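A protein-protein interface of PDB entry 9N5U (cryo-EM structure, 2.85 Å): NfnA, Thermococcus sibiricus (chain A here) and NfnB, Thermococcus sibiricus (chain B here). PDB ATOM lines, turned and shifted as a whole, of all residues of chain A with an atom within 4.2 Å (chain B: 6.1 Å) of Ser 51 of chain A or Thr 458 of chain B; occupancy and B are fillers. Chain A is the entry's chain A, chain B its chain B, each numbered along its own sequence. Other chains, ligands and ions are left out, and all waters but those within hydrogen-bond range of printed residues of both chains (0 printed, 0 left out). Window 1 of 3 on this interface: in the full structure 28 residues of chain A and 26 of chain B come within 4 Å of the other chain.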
ATOM      1  N   CYS A  41      11.900   3.066  25.410  1.00  0.00           N
ATOM      2  CA  CYS A  41      11.700   3.317  26.829  1.00  0.00           C
ATOM      3  C   CYS A  41      10.494   2.614  27.439  1.00  0.00           C
ATOM      4  O   CYS A  41      10.290   2.728  28.649  1.00  0.00           O
ATOM      5  CB  CYS A  41      11.576   4.821  27.067  1.00  0.00           C
ATOM      6  SG  CYS A  41      10.405   5.641  25.979  1.00  0.00           S
ATOM      7  N   TYR A  49       6.446   5.748  29.606  1.00  0.00           N
ATOM      8  CA  TYR A  49       7.486   6.760  29.678  1.00  0.00           C
ATOM      9  C   TYR A  49       7.626   7.350  28.283  1.00  0.00           C
ATOM     10  O   TYR A  49       7.679   6.605  27.301  1.00  0.00           O
ATOM     11  CB  TYR A  49       8.798   6.119  30.141  1.00  0.00           C
ATOM     12  CG  TYR A  49       9.774   6.988  30.902  1.00  0.00           C
ATOM     13  CD1 TYR A  49       9.517   7.387  32.204  1.00  0.00           C
ATOM     14  CD2 TYR A  49      10.988   7.351  30.337  1.00  0.00           C
ATOM     15  CE1 TYR A  49      10.425   8.155  32.904  1.00  0.00           C
ATOM     16  CE2 TYR A  49      11.896   8.118  31.027  1.00  0.00           C
ATOM     17  CZ  TYR A  49      11.613   8.514  32.309  1.00  0.00           C
ATOM     18  OH  TYR A  49      12.522   9.276  32.996  1.00  0.00           O
ATOM     19  N   GLY A  50       7.665   8.673  28.188  1.00  0.00           N
ATOM     20  CA  GLY A  50       7.685   9.315  26.887  1.00  0.00           C
ATOM     21  C   GLY A  50       9.024   9.889  26.468  1.00  0.00           C
ATOM     22  O   GLY A  50       9.081  11.011  25.959  1.00  0.00           O
ATOM     23  N   SER A  51      10.108   9.142  26.669  1.00  0.00           N
ATOM     24  CA  SER A  51      11.440   9.701  26.468  1.00  0.00           C
ATOM     25  C   SER A  51      12.017   9.436  25.079  1.00  0.00           C
ATOM     26  O   SER A  51      12.675  10.313  24.514  1.00  0.00           O
ATOM     27  CB  SER A  51      12.396   9.159  27.530  1.00  0.00           C
ATOM     28  OG  SER A  51      12.641   7.781  27.340  1.00  0.00           O
ATOM     29  N   CYS A  52      11.813   8.249  24.511  1.00  0.00           N
ATOM     30  CA  CYS A  52      12.461   7.949  23.238  1.00  0.00           C
ATOM     31  C   CYS A  52      11.769   8.624  22.060  1.00  0.00           C
ATOM     32  O   CYS A  52      12.437   8.980  21.085  1.00  0.00           O
ATOM     33  CB  CYS A  52      12.532   6.438  23.019  1.00  0.00           C
ATOM     34  SG  CYS A  52      11.068   5.690  22.319  1.00  0.00           S
ATOM     35  N   ARG A  53      10.447   8.805  22.138  1.00  0.00           N
ATOM     36  CA  ARG A  53       9.653   9.499  21.117  1.00  0.00           C
ATOM     37  C   ARG A  53       9.753   8.820  19.752  1.00  0.00           C
ATOM     38  O   ARG A  53       9.827   9.483  18.718  1.00  0.00           O
ATOM     39  CB  ARG A  53      10.051  10.971  21.010  1.00  0.00           C
ATOM     40  CG  ARG A  53      10.155  11.694  22.337  1.00  0.00           C
ATOM     41  CD  ARG A  53       8.862  12.384  22.699  1.00  0.00           C
ATOM     42  NE  ARG A  53       7.939  11.550  23.452  1.00  0.00           N
ATOM     43  CZ  ARG A  53       6.631  11.757  23.516  1.00  0.00           C
ATOM     44  NH1 ARG A  53       6.048  12.715  22.817  1.00  0.00           N
ATOM     45  NH2 ARG A  53       5.889  10.978  24.296  1.00  0.00           N
ATOM     46  N   ILE A  95      19.394  11.170  17.686  1.00  0.00           N
ATOM     47  CA  ILE A  95      20.033  10.278  18.649  1.00  0.00           C
ATOM     48  C   ILE A  95      21.442   9.912  18.196  1.00  0.00           C
ATOM     49  O   ILE A  95      22.380   9.877  18.999  1.00  0.00           O
ATOM     50  CB  ILE A  95      19.162   9.028  18.875  1.00  0.00           C
ATOM     51  CG1 ILE A  95      17.835   9.412  19.525  1.00  0.00           C
ATOM     52  CG2 ILE A  95      19.884   8.016  19.734  1.00  0.00           C
ATOM     53  CD1 ILE A  95      16.898   8.252  19.726  1.00  0.00           C
ATOM     54  N   LEU A 642      19.383   7.599  26.750  1.00  0.00           N
ATOM     55  CA  LEU A 642      18.577   8.230  27.797  1.00  0.00           C
ATOM     56  C   LEU A 642      17.101   7.837  27.670  1.00  0.00           C
ATOM     57  O   LEU A 642      16.226   8.652  27.383  1.00  0.00           O
ATOM     58  CB  LEU A 642      18.750   9.753  27.787  1.00  0.00           C
ATOM     59  CG  LEU A 642      19.990  10.301  28.487  1.00  0.00           C
ATOM     60  CD1 LEU A 642      20.076  11.798  28.305  1.00  0.00           C
ATOM     61  CD2 LEU A 642      19.961   9.950  29.957  1.00  0.00           C
ATOM     62  N   CYS A 643      16.855   6.549  27.890  1.00  0.00           N
ATOM     63  CA  CYS A 643      15.496   6.032  27.911  1.00  0.00           C
ATOM     64  C   CYS A 643      14.932   5.884  29.317  1.00  0.00           C
ATOM     65  O   CYS A 643      13.712   5.778  29.468  1.00  0.00           O
ATOM     66  CB  CYS A 643      15.427   4.684  27.183  1.00  0.00           C
ATOM     67  SG  CYS A 643      16.494   3.398  27.841  1.00  0.00           S
ATOM     68  N   LYS B 456      14.629  14.894  29.012  1.00  0.00           N
ATOM     69  CA  LYS B 456      13.947  13.610  29.089  1.00  0.00           C
ATOM     70  C   LYS B 456      13.635  13.033  27.715  1.00  0.00           C
ATOM     71  O   LYS B 456      14.036  11.907  27.413  1.00  0.00           O
ATOM     72  CB  LYS B 456      12.659  13.740  29.909  1.00  0.00           C
ATOM     73  CG  LYS B 456      11.875  12.455  30.025  1.00  0.00           C
ATOM     74  CD  LYS B 456      10.688  12.612  30.951  1.00  0.00           C
ATOM     75  CE  LYS B 456       9.849  11.356  30.978  1.00  0.00           C
ATOM     76  NZ  LYS B 456       8.763  11.447  31.975  1.00  0.00           N
ATOM     77  N   CYS B 457      12.936  13.779  26.869  1.00  0.00           N
ATOM     78  CA  CYS B 457      12.583  13.279  25.552  1.00  0.00           C
ATOM     79  C   CYS B 457      13.663  13.638  24.539  1.00  0.00           C
ATOM     80  O   CYS B 457      14.329  14.670  24.648  1.00  0.00           O
ATOM     81  CB  CYS B 457      11.220  13.808  25.103  1.00  0.00           C
ATOM     82  SG  CYS B 457      11.121  15.557  24.740  1.00  0.00           S
ATOM     83  N   THR B 458      13.841  12.754  23.557  1.00  0.00           N
ATOM     84  CA  THR B 458      14.930  12.917  22.599  1.00  0.00           C
ATOM     85  C   THR B 458      14.744  14.169  21.752  1.00  0.00           C
ATOM     86  O   THR B 458      15.718  14.866  21.447  1.00  0.00           O
ATOM     87  CB  THR B 458      15.044  11.680  21.707  1.00  0.00           C
ATOM     88  OG1 THR B 458      13.821  11.488  20.989  1.00  0.00           O
ATOM     89  CG2 THR B 458      15.325  10.451  22.541  1.00  0.00           C
ATOM     90  N   PHE B 459      13.500  14.472  21.375  1.00  0.00           N
ATOM     91  CA  PHE B 459      13.242  15.584  20.467  1.00  0.00           C
ATOM     92  C   PHE B 459      13.632  16.921  21.082  1.00  0.00           C
ATOM     93  O   PHE B 459      14.410  17.668  20.493  1.00  0.00           O
ATOM     94  CB  PHE B 459      11.776  15.594  20.048  1.00  0.00           C
ATOM     95  CG  PHE B 459      11.516  14.871  18.766  1.00  0.00           C
ATOM     96  CD1 PHE B 459      11.927  15.411  17.563  1.00  0.00           C
ATOM     97  CD2 PHE B 459      10.862  13.655  18.761  1.00  0.00           C
ATOM     98  CE1 PHE B 459      11.690  14.754  16.381  1.00  0.00           C
ATOM     99  CE2 PHE B 459      10.620  12.993  17.581  1.00  0.00           C
ATOM    100  CZ  PHE B 459      11.035  13.543  16.390  1.00  0.00           C
ATOM    101  N   CYS B 460      13.128  17.235  22.276  1.00  0.00           N
ATOM    102  CA  CYS B 460      13.487  18.511  22.891  1.00  0.00           C
ATOM    103  C   CYS B 460      14.983  18.573  23.169  1.00  0.00           C
ATOM    104  O   CYS B 460      15.683  19.449  22.647  1.00  0.00           O
ATOM    105  CB  CYS B 460      12.685  18.723  24.176  1.00  0.00           C
ATOM    106  SG  CYS B 460      13.070  20.236  25.090  1.00  0.00           S
ATOM    107  N   ARG B 461      15.501  17.563  23.877  1.00  0.00           N
ATOM    108  CA  ARG B 461      16.883  17.571  24.347  1.00  0.00           C
ATOM    109  C   ARG B 461      17.870  17.704  23.196  1.00  0.00           C
ATOM    110  O   ARG B 461      18.831  18.477  23.280  1.00  0.00           O
ATOM    111  CB  ARG B 461      17.162  16.292  25.140  1.00  0.00           C
ATOM    112  CG  ARG B 461      18.584  16.161  25.648  1.00  0.00           C
ATOM    113  CD  ARG B 461      18.817  14.851  26.393  1.00  0.00           C
ATOM    114  NE  ARG B 461      19.041  13.722  25.498  1.00  0.00           N
ATOM    115  CZ  ARG B 461      18.183  12.729  25.311  1.00  0.00           C
ATOM    116  NH1 ARG B 461      17.034  12.675  25.960  1.00  0.00           N
ATOM    117  NH2 ARG B 461      18.487  11.763  24.449  1.00  0.00           N
ATOM    118  N   LEU B 462      17.638  16.979  22.106  1.00  0.00           N
ATOM    119  CA  LEU B 462      18.591  16.972  21.007  1.00  0.00           C
ATOM    120  C   LEU B 462      18.270  18.011  19.937  1.00  0.00           C
ATOM    121  O   LEU B 462      19.175  18.705  19.463  1.00  0.00           O
ATOM    122  CB  LEU B 462      18.649  15.572  20.394  1.00  0.00           C
ATOM    123  CG  LEU B 462      19.098  14.503  21.392  1.00  0.00           C
ATOM    124  CD1 LEU B 462      18.851  13.104  20.864  1.00  0.00           C
ATOM    125  CD2 LEU B 462      20.563  14.693  21.744  1.00  0.00           C
ATOM    126  N   GLY B 463      17.002  18.124  19.536  1.00  0.00           N
ATOM    127  CA  GLY B 463      16.627  19.063  18.505  1.00  0.00           C
ATOM    128  C   GLY B 463      16.790  20.514  18.899  1.00  0.00           C
ATOM    129  O   GLY B 463      17.106  21.344  18.047  1.00  0.00           O
ATOM    130  N   LEU B 499       7.460  15.987  24.140  1.00  0.00           N
ATOM    131  CA  LEU B 499       6.510  15.452  25.107  1.00  0.00           C
ATOM    132  C   LEU B 499       5.779  16.537  25.887  1.00  0.00           C
ATOM    133  O   LEU B 499       4.562  16.444  26.077  1.00  0.00           O
ATOM    134  CB  LEU B 499       7.231  14.517  26.080  1.00  0.00           C
ATOM    135  CG  LEU B 499       6.438  14.014  27.285  1.00  0.00           C
ATOM    136  CD1 LEU B 499       5.328  13.083  26.849  1.00  0.00           C
ATOM    137  CD2 LEU B 499       7.358  13.326  28.266  1.00  0.00           C
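The backbone carbonyl oxygen of Ser 51 of chain A sits at hydrogen-bond distance from the backbone NH of Thr 458 of chain B (2.9 Å). The backbone carbonyl oxygen (O) of Cys 52 of chain A lies within hydrogen-bond range of the side-chain hydroxyl (OG1) of Thr 458 of chain B (2.9 Å).
Ser 51 of chain A touches just these residues of chain B: Lys 456 (3.2 Å), Cys 457 (3.1 Å) and Thr 458 (2.9 Å). Of the printed residues of chain A, Thr 458 of chain B touches Ser 51 (2.9 Å), Cys 52 (2.9 Å), Arg 53 (3.8 Å) and Ile 95 (3.9 Å). Printed residues of chain A within 4 Å of Phe 459 of chain B: Arg 53. Printed residues of chain A within 4 Å of Cys 457 of chain B: Gly 50, Ser 51 and Arg 53. Printed residues of chain A within 4 Å of Leu 499 of chain B: Gly 50 and Arg 53. Of the printed residues of chain B, Gly 50 of chain A touches Cys 457 and Leu 499. Cys 643 of chain A touches none of the printed residues of chain B. Gly 463 of chain B touches none of the printed residues of chain A. The nearest printed residue of chain A that does not touch Thr 458 of chain B is Leu 642 of chain A (5.2 Å).
CE of Lys 456 of chain B touches CZ of Tyr 49 of chain A, at 3.6 Å. Gly 50 of chain A touches Leu 499 of chain B (O to CD2, 3.7 Å). Ser 51 of chain A touches Lys 456 of chain B (CB to O, 3.2 Å). Ser 51 of chain A touches Cys 457 of chain B. CG of Arg 53 of chain A touches CB of Cys 457 of chain B (3.6 Å). Arg 53 of chain A touches Thr 458 of chain B (CB to OG1, 3.8 Å). CB of Arg 53 of chain A touches CD2 of Phe 459 of chain B (3.6 Å). Arg 53 of chain A touches Leu 499 of chain B. Thr 458 of chain B touches Ile 95 of chain A. N of Ile 95 of chain A touches CD1 of Leu 462 of chain B (3.8 Å).
Of the 9 printed residues of chain B, 7 touch a printed residue of chain A. Printed residues of chain B that touch a printed residue of chain A: Lys 456, Cys 457, Thr 458, Phe 459, Arg 461, Leu 462 and Leu 499. Hydrophobic or aromatic side chains of chain B within 4 Å of the printed part of chain A: Phe 459, Leu 462 and Leu 499. Among the printed residues, 15 pairs touch across the chains. Among the printed residues, no Asp or Glu carboxylate lies within 4 Å of a Lys or Arg side-chain nitrogen of the other chain.
The side-chain sulfur (SG) of Cys 41 of chain A lies close to the backbone carbonyl oxygen (O) of Tyr 49 of chain A (3.2 Å). The backbone carbonyl oxygen (O) of Gly 50 of chain A lies within hydrogen-bond range of the guanidinium group (NE) of Arg 53 of chain A, 2.8 Å away. OG of Ser 51 of chain A sits at hydrogen-bond distance from O of Cys 643 of chain A, at 3.1 Å. The backbone carbonyl oxygen of Lys 456 of chain B lies within hydrogen-bond range of the guanidinium group of Arg 461 of chain B (3.4 Å). The backbone NH of Cys 460 of chain B lies close to the side-chain sulfur of Cys 457 of chain B. The side-chain sulfur of Cys 457 of chain B sits close to the backbone NH of Leu 499 of chain B (3.7 Å).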
